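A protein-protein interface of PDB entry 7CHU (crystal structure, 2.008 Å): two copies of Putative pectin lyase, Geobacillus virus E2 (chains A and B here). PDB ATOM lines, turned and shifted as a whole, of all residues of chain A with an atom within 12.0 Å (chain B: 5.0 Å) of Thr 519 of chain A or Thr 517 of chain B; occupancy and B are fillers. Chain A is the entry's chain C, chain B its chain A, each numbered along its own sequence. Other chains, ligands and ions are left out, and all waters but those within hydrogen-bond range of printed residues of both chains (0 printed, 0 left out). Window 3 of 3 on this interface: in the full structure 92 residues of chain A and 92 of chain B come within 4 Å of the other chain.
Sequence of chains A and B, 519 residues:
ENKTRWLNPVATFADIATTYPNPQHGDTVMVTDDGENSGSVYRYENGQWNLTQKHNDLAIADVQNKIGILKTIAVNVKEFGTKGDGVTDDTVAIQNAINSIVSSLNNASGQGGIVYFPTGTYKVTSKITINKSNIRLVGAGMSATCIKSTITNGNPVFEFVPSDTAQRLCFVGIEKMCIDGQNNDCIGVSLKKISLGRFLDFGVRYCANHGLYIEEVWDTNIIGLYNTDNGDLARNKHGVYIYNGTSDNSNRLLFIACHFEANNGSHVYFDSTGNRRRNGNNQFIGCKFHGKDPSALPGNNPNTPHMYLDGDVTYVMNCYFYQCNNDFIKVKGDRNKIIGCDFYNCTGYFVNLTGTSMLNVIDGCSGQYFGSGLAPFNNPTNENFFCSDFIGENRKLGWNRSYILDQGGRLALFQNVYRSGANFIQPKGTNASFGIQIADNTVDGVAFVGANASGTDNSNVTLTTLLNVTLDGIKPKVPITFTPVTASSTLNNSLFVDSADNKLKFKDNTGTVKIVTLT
OXT of Thr 519 of chain A lies within salt-bridge range of NZ of Lys 514 of chain B, 3.9 Å away. O of Thr 519 of chain A sits at hydrogen-bond distance from N of Ile 515 of chain B, at 2.9 Å. N of Thr 517 of chain B is in hydrogen-bond range of O of Thr 517 of chain A. The side-chain hydroxyl of Thr 517 of chain B lies within hydrogen-bond range of the side-chain hydroxyl of Thr 519 of chain A (3.3 Å).
O of Leu 504 of chain A sits at hydrogen-bond distance from N of Val 516 of chain A (3.1 Å).
Among the printed residues, merely in contact across the chains: Val 516 of chain A with Val 516 of chain B, Leu 518 of chain A with Lys 514 of chain B, Leu 518 of chain A with Ile 515 of chain B, Leu 518 of chain A with Val 516 of chain B and Leu 518 of chain A with Thr 517 of chain B.
Lys 503 of chain A touches none of the printed residues of chain B. Ile 515 of chain A touches none of the printed residues of chain B. Of the printed residues of chain B, Val 516 of chain A touches Val 516 (3.9 Å). Of the printed residues of chain B, Thr 517 of chain A touches Thr 517. Of the printed residues of chain B, Leu 518 of chain A touches Lys 514, Ile 515, Val 516 and Thr 517. Thr 519 of chain A touches just these residues of chain B: Lys 514, Ile 515 and Thr 517. Lys 514 of chain B touches two residues of chain A. Ile 515 of chain B touches two residues of chain A. Of the printed residues of chain A, Val 516 of chain B touches Val 516 (3.9 Å) and Leu 518 (3.99 Å). Thr 517 of chain B touches three residues of chain A. No residue of chain A comes within 4 Å of Leu 518 of chain B. No residue of chain A comes within 4 Å of Thr 519 of chain B. The nearest printed residue of chain B that does not touch Thr 519 of chain A is Val 516 of chain B (5.1 Å). The nearest printed residue of chain B that does not touch Leu 518 of chain A is Leu 518 of chain B (7.9 Å).
Of the 6 printed residues of chain B, 4 touch a printed residue of chain A. Of the 11 printed residues of chain A, 4 touch a printed residue of chain B. Among the printed residues, 9 pairs touch across the chains.
Thr 517 of chain B touches its own counterpart, Thr 517 of chain A. Leu 518 of chain A touches Ile 515 of chain B, but with the chains exchanged Ile 515 of chain A does not touch Leu 518 of chain B (10.5 Å). Leu 518 of chain A touches Val 516 of chain B, but with the chains exchanged Val 516 of chain A does not touch Leu 518 of chain B (7.6 Å). Thr 519 of chain A touches Thr 517 of chain B, but with the chains exchanged Thr 517 of chain A does not touch Thr 519 of chain B (7.8 Å). Positions printed for both chains: 514, 515, 516, 517, 518 and 519. Of the 9 pairs that touch across the chains among the printed residues, 2 have their exchanged pair printed and touching as well.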
ATOM      1  N   LEU A 495     -30.801 -16.927  19.407  1.00  0.00           N
ATOM      2  CA  LEU A 495     -30.375 -18.040  18.580  1.00  0.00           C
ATOM      3  C   LEU A 495     -31.435 -19.132  18.658  1.00  0.00           C
ATOM      4  O   LEU A 495     -31.843 -19.507  19.761  1.00  0.00           O
ATOM      5  CB  LEU A 495     -29.024 -18.553  19.094  1.00  0.00           C
ATOM      6  CG  LEU A 495     -28.241 -19.545  18.251  1.00  0.00           C
ATOM      7  CD1 LEU A 495     -27.996 -18.951  16.869  1.00  0.00           C
ATOM      8  CD2 LEU A 495     -26.921 -19.892  18.944  1.00  0.00           C
ATOM      9  N   LYS A 503     -33.642 -24.064   9.568  1.00  0.00           N
ATOM     10  CA  LYS A 503     -32.293 -23.519   9.511  1.00  0.00           C
ATOM     11  C   LYS A 503     -31.957 -22.831  10.827  1.00  0.00           C
ATOM     12  O   LYS A 503     -32.822 -22.193  11.434  1.00  0.00           O
ATOM     13  CB  LYS A 503     -32.151 -22.528   8.359  1.00  0.00           C
ATOM     14  CG  LYS A 503     -32.311 -23.110   6.947  1.00  0.00           C
ATOM     15  CD  LYS A 503     -32.187 -21.959   5.925  1.00  0.00           C
ATOM     16  CE  LYS A 503     -32.493 -22.329   4.472  1.00  0.00           C
ATOM     17  NZ  LYS A 503     -32.576 -21.064   3.609  1.00  0.00           N
ATOM     18  N   LEU A 504     -30.695 -22.963  11.259  1.00  0.00           N
ATOM     19  CA  LEU A 504     -30.198 -22.212  12.410  1.00  0.00           C
ATOM     20  C   LEU A 504     -30.131 -20.719  12.093  1.00  0.00           C
ATOM     21  O   LEU A 504     -29.493 -20.300  11.117  1.00  0.00           O
ATOM     22  CB  LEU A 504     -28.816 -22.718  12.817  1.00  0.00           C
ATOM     23  CG  LEU A 504     -28.164 -22.059  14.030  1.00  0.00           C
ATOM     24  CD1 LEU A 504     -28.901 -22.448  15.297  1.00  0.00           C
ATOM     25  CD2 LEU A 504     -26.678 -22.427  14.121  1.00  0.00           C
ATOM     26  N   LYS A 505     -30.775 -19.905  12.922  1.00  0.00           N
ATOM     27  CA  LYS A 505     -30.871 -18.483  12.632  1.00  0.00           C
ATOM     28  C   LYS A 505     -30.602 -17.696  13.897  1.00  0.00           C
ATOM     29  O   LYS A 505     -30.657 -18.238  15.006  1.00  0.00           O
ATOM     30  CB  LYS A 505     -32.248 -18.116  12.044  1.00  0.00           C
ATOM     31  CG  LYS A 505     -32.534 -18.820  10.705  1.00  0.00           C
ATOM     32  CD  LYS A 505     -33.792 -18.293  10.064  1.00  0.00           C
ATOM     33  CE  LYS A 505     -34.157 -19.079   8.815  1.00  0.00           C
ATOM     34  NZ  LYS A 505     -35.481 -18.629   8.333  1.00  0.00           N
ATOM     35  N   PHE A 506     -30.274 -16.410  13.708  1.00  0.00           N
ATOM     36  CA  PHE A 506     -30.044 -15.473  14.804  1.00  0.00           C
ATOM     37  C   PHE A 506     -30.854 -14.214  14.527  1.00  0.00           C
ATOM     38  O   PHE A 506     -30.702 -13.600  13.465  1.00  0.00           O
ATOM     39  CB  PHE A 506     -28.551 -15.136  14.932  1.00  0.00           C
ATOM     40  CG  PHE A 506     -28.219 -14.237  16.097  1.00  0.00           C
ATOM     41  CD1 PHE A 506     -28.179 -14.744  17.397  1.00  0.00           C
ATOM     42  CD2 PHE A 506     -27.938 -12.895  15.901  1.00  0.00           C
ATOM     43  CE1 PHE A 506     -27.893 -13.930  18.460  1.00  0.00           C
ATOM     44  CE2 PHE A 506     -27.642 -12.081  16.964  1.00  0.00           C
ATOM     45  CZ  PHE A 506     -27.621 -12.596  18.242  1.00  0.00           C
ATOM     46  N   LYS A 514     -31.460 -13.286  10.828  1.00  0.00           N
ATOM     47  CA  LYS A 514     -30.373 -13.610   9.914  1.00  0.00           C
ATOM     48  C   LYS A 514     -30.049 -15.095  10.005  1.00  0.00           C
ATOM     49  O   LYS A 514     -30.284 -15.733  11.033  1.00  0.00           O
ATOM     50  CB  LYS A 514     -29.134 -12.783  10.222  1.00  0.00           C
ATOM     51  CG  LYS A 514     -29.418 -11.279  10.281  1.00  0.00           C
ATOM     52  CD  LYS A 514     -28.145 -10.485  10.110  1.00  0.00           C
ATOM     53  CE  LYS A 514     -27.653 -10.509   8.671  1.00  0.00           C
ATOM     54  NZ  LYS A 514     -26.660  -9.403   8.448  1.00  0.00           N
ATOM     55  N   ILE A 515     -29.515 -15.642   8.922  1.00  0.00           N
ATOM     56  CA  ILE A 515     -29.167 -17.055   8.846  1.00  0.00           C
ATOM     57  C   ILE A 515     -27.727 -17.230   9.301  1.00  0.00           C
ATOM     58  O   ILE A 515     -26.849 -16.453   8.911  1.00  0.00           O
ATOM     59  CB  ILE A 515     -29.368 -17.587   7.414  1.00  0.00           C
ATOM     60  CG1 ILE A 515     -30.862 -17.616   7.079  1.00  0.00           C
ATOM     61  CG2 ILE A 515     -28.748 -18.964   7.251  1.00  0.00           C
ATOM     62  CD1 ILE A 515     -31.148 -17.927   5.638  1.00  0.00           C
ATOM     63  N   VAL A 516     -27.476 -18.226  10.149  1.00  0.00           N
ATOM     64  CA  VAL A 516     -26.103 -18.514  10.549  1.00  0.00           C
ATOM     65  C   VAL A 516     -25.422 -19.256   9.402  1.00  0.00           C
ATOM     66  O   VAL A 516     -25.862 -20.335   8.997  1.00  0.00           O
ATOM     67  CB  VAL A 516     -26.051 -19.314  11.859  1.00  0.00           C
ATOM     68  CG1 VAL A 516     -24.593 -19.619  12.249  1.00  0.00           C
ATOM     69  CG2 VAL A 516     -26.774 -18.549  12.989  1.00  0.00           C
ATOM     70  N   THR A 517     -24.347 -18.671   8.873  1.00  0.00           N
ATOM     71  CA  THR A 517     -23.613 -19.288   7.779  1.00  0.00           C
ATOM     72  C   THR A 517     -22.939 -20.587   8.218  1.00  0.00           C
ATOM     73  O   THR A 517     -22.157 -20.607   9.167  1.00  0.00           O
ATOM     74  CB  THR A 517     -22.556 -18.316   7.245  1.00  0.00           C
ATOM     75  OG1 THR A 517     -23.206 -17.118   6.818  1.00  0.00           O
ATOM     76  CG2 THR A 517     -21.823 -18.923   6.069  1.00  0.00           C
ATOM     77  N   LEU A 518     -23.222 -21.666   7.504  1.00  0.00           N
ATOM     78  CA  LEU A 518     -22.631 -22.967   7.765  1.00  0.00           C
ATOM     79  C   LEU A 518     -21.801 -23.399   6.569  1.00  0.00           C
ATOM     80  O   LEU A 518     -22.217 -23.220   5.419  1.00  0.00           O
ATOM     81  CB  LEU A 518     -23.711 -24.016   8.040  1.00  0.00           C
ATOM     82  CG  LEU A 518     -24.589 -23.720   9.248  1.00  0.00           C
ATOM     83  CD1 LEU A 518     -25.650 -24.808   9.418  1.00  0.00           C
ATOM     84  CD2 LEU A 518     -23.739 -23.602  10.505  1.00  0.00           C
ATOM     85  N   THR A 519     -20.643 -23.980   6.839  1.00  0.00           N
ATOM     86  CA  THR A 519     -19.863 -24.608   5.784  1.00  0.00           C
ATOM     87  C   THR A 519     -19.845 -26.139   5.906  1.00  0.00           C
ATOM     88  O   THR A 519     -19.652 -26.715   7.000  1.00  0.00           O
ATOM     89  CB  THR A 519     -18.432 -24.083   5.782  1.00  0.00           C
ATOM     90  OG1 THR A 519     -18.433 -22.761   5.225  1.00  0.00           O
ATOM     91  CG2 THR A 519     -17.536 -24.983   4.952  1.00  0.00           C
ATOM     92  OXT THR A 519     -20.039 -26.818   4.883  1.00  0.00           O
ATOM     93  N   LYS B 514     -21.932 -29.602  10.253  1.00  0.00           N
ATOM     94  CA  LYS B 514     -21.370 -28.486   9.507  1.00  0.00           C
ATOM     95  C   LYS B 514     -20.562 -27.587  10.434  1.00  0.00           C
ATOM     96  O   LYS B 514     -20.832 -27.512  11.636  1.00  0.00           O
ATOM     97  CB  LYS B 514     -22.472 -27.685   8.822  1.00  0.00           C
ATOM     98  CG  LYS B 514     -23.432 -28.584   8.065  1.00  0.00           C
ATOM     99  CD  LYS B 514     -24.381 -27.799   7.238  1.00  0.00           C
ATOM    100  CE  LYS B 514     -23.741 -27.382   5.946  1.00  0.00           C
ATOM    101  NZ  LYS B 514     -23.479 -28.582   5.106  1.00  0.00           N
ATOM    102  N   ILE B 515     -19.572 -26.904   9.860  1.00  0.00           N
ATOM    103  CA  ILE B 515     -18.759 -25.949  10.606  1.00  0.00           C
ATOM    104  C   ILE B 515     -19.503 -24.622  10.668  1.00  0.00           C
ATOM    105  O   ILE B 515     -20.067 -24.175   9.667  1.00  0.00           O
ATOM    106  CB  ILE B 515     -17.370 -25.793   9.960  1.00  0.00           C
ATOM    107  CG1 ILE B 515     -16.526 -27.039  10.271  1.00  0.00           C
ATOM    108  CG2 ILE B 515     -16.677 -24.505  10.461  1.00  0.00           C
ATOM    109  CD1 ILE B 515     -15.196 -27.102   9.565  1.00  0.00           C
ATOM    110  N   VAL B 516     -19.574 -24.025  11.856  1.00  0.00           N
ATOM    111  CA  VAL B 516     -20.148 -22.690  11.981  1.00  0.00           C
ATOM    112  C   VAL B 516     -19.096 -21.687  11.513  1.00  0.00           C
ATOM    113  O   VAL B 516     -18.003 -21.611  12.083  1.00  0.00           O
ATOM    114  CB  VAL B 516     -20.589 -22.401  13.421  1.00  0.00           C
ATOM    115  CG1 VAL B 516     -21.111 -20.982  13.517  1.00  0.00           C
ATOM    116  CG2 VAL B 516     -21.657 -23.411  13.899  1.00  0.00           C
ATOM    117  N   THR B 517     -19.417 -20.934  10.466  1.00  0.00           N
ATOM    118  CA  THR B 517     -18.424 -20.062   9.839  1.00  0.00           C
ATOM    119  C   THR B 517     -18.105 -18.860  10.725  1.00  0.00           C
ATOM    120  O   THR B 517     -19.003 -18.127  11.154  1.00  0.00           O
ATOM    121  CB  THR B 517     -18.927 -19.576   8.481  1.00  0.00           C
ATOM    122  OG1 THR B 517     -19.170 -20.697   7.630  1.00  0.00           O
ATOM    123  CG2 THR B 517     -17.906 -18.649   7.824  1.00  0.00           C
ATOM    124  N   LEU B 518     -16.815 -18.635  10.948  1.00  0.00           N
ATOM    125  CA  LEU B 518     -16.309 -17.532  11.744  1.00  0.00           C
ATOM    126  C   LEU B 518     -15.420 -16.640  10.885  1.00  0.00           C
ATOM    127  O   LEU B 518     -14.697 -17.130  10.015  1.00  0.00           O
ATOM    128  CB  LEU B 518     -15.490 -18.055  12.937  1.00  0.00           C
ATOM    129  CG  LEU B 518     -16.135 -19.194  13.744  1.00  0.00           C
ATOM    130  CD1 LEU B 518     -15.148 -19.772  14.746  1.00  0.00           C
ATOM    131  CD2 LEU B 518     -17.395 -18.687  14.435  1.00  0.00           C
ATOM    132  N   THR B 519     -15.447 -15.333  11.144  1.00  0.00           N
ATOM    133  CA  THR B 519     -14.466 -14.449  10.480  1.00  0.00           C
ATOM    134  C   THR B 519     -13.469 -13.810  11.462  1.00  0.00           C
ATOM    135  O   THR B 519     -12.265 -13.773  11.190  1.00  0.00           O
ATOM    136  CB  THR B 519     -15.134 -13.301   9.684  1.00  0.00           C
ATOM    137  OG1 THR B 519     -15.367 -12.180  10.546  1.00  0.00           O
ATOM    138  CG2 THR B 519     -16.448 -13.744   9.075  1.00  0.00           C
ATOM    139  OXT THR B 519     -13.823 -13.304  12.535  1.00  0.00           O
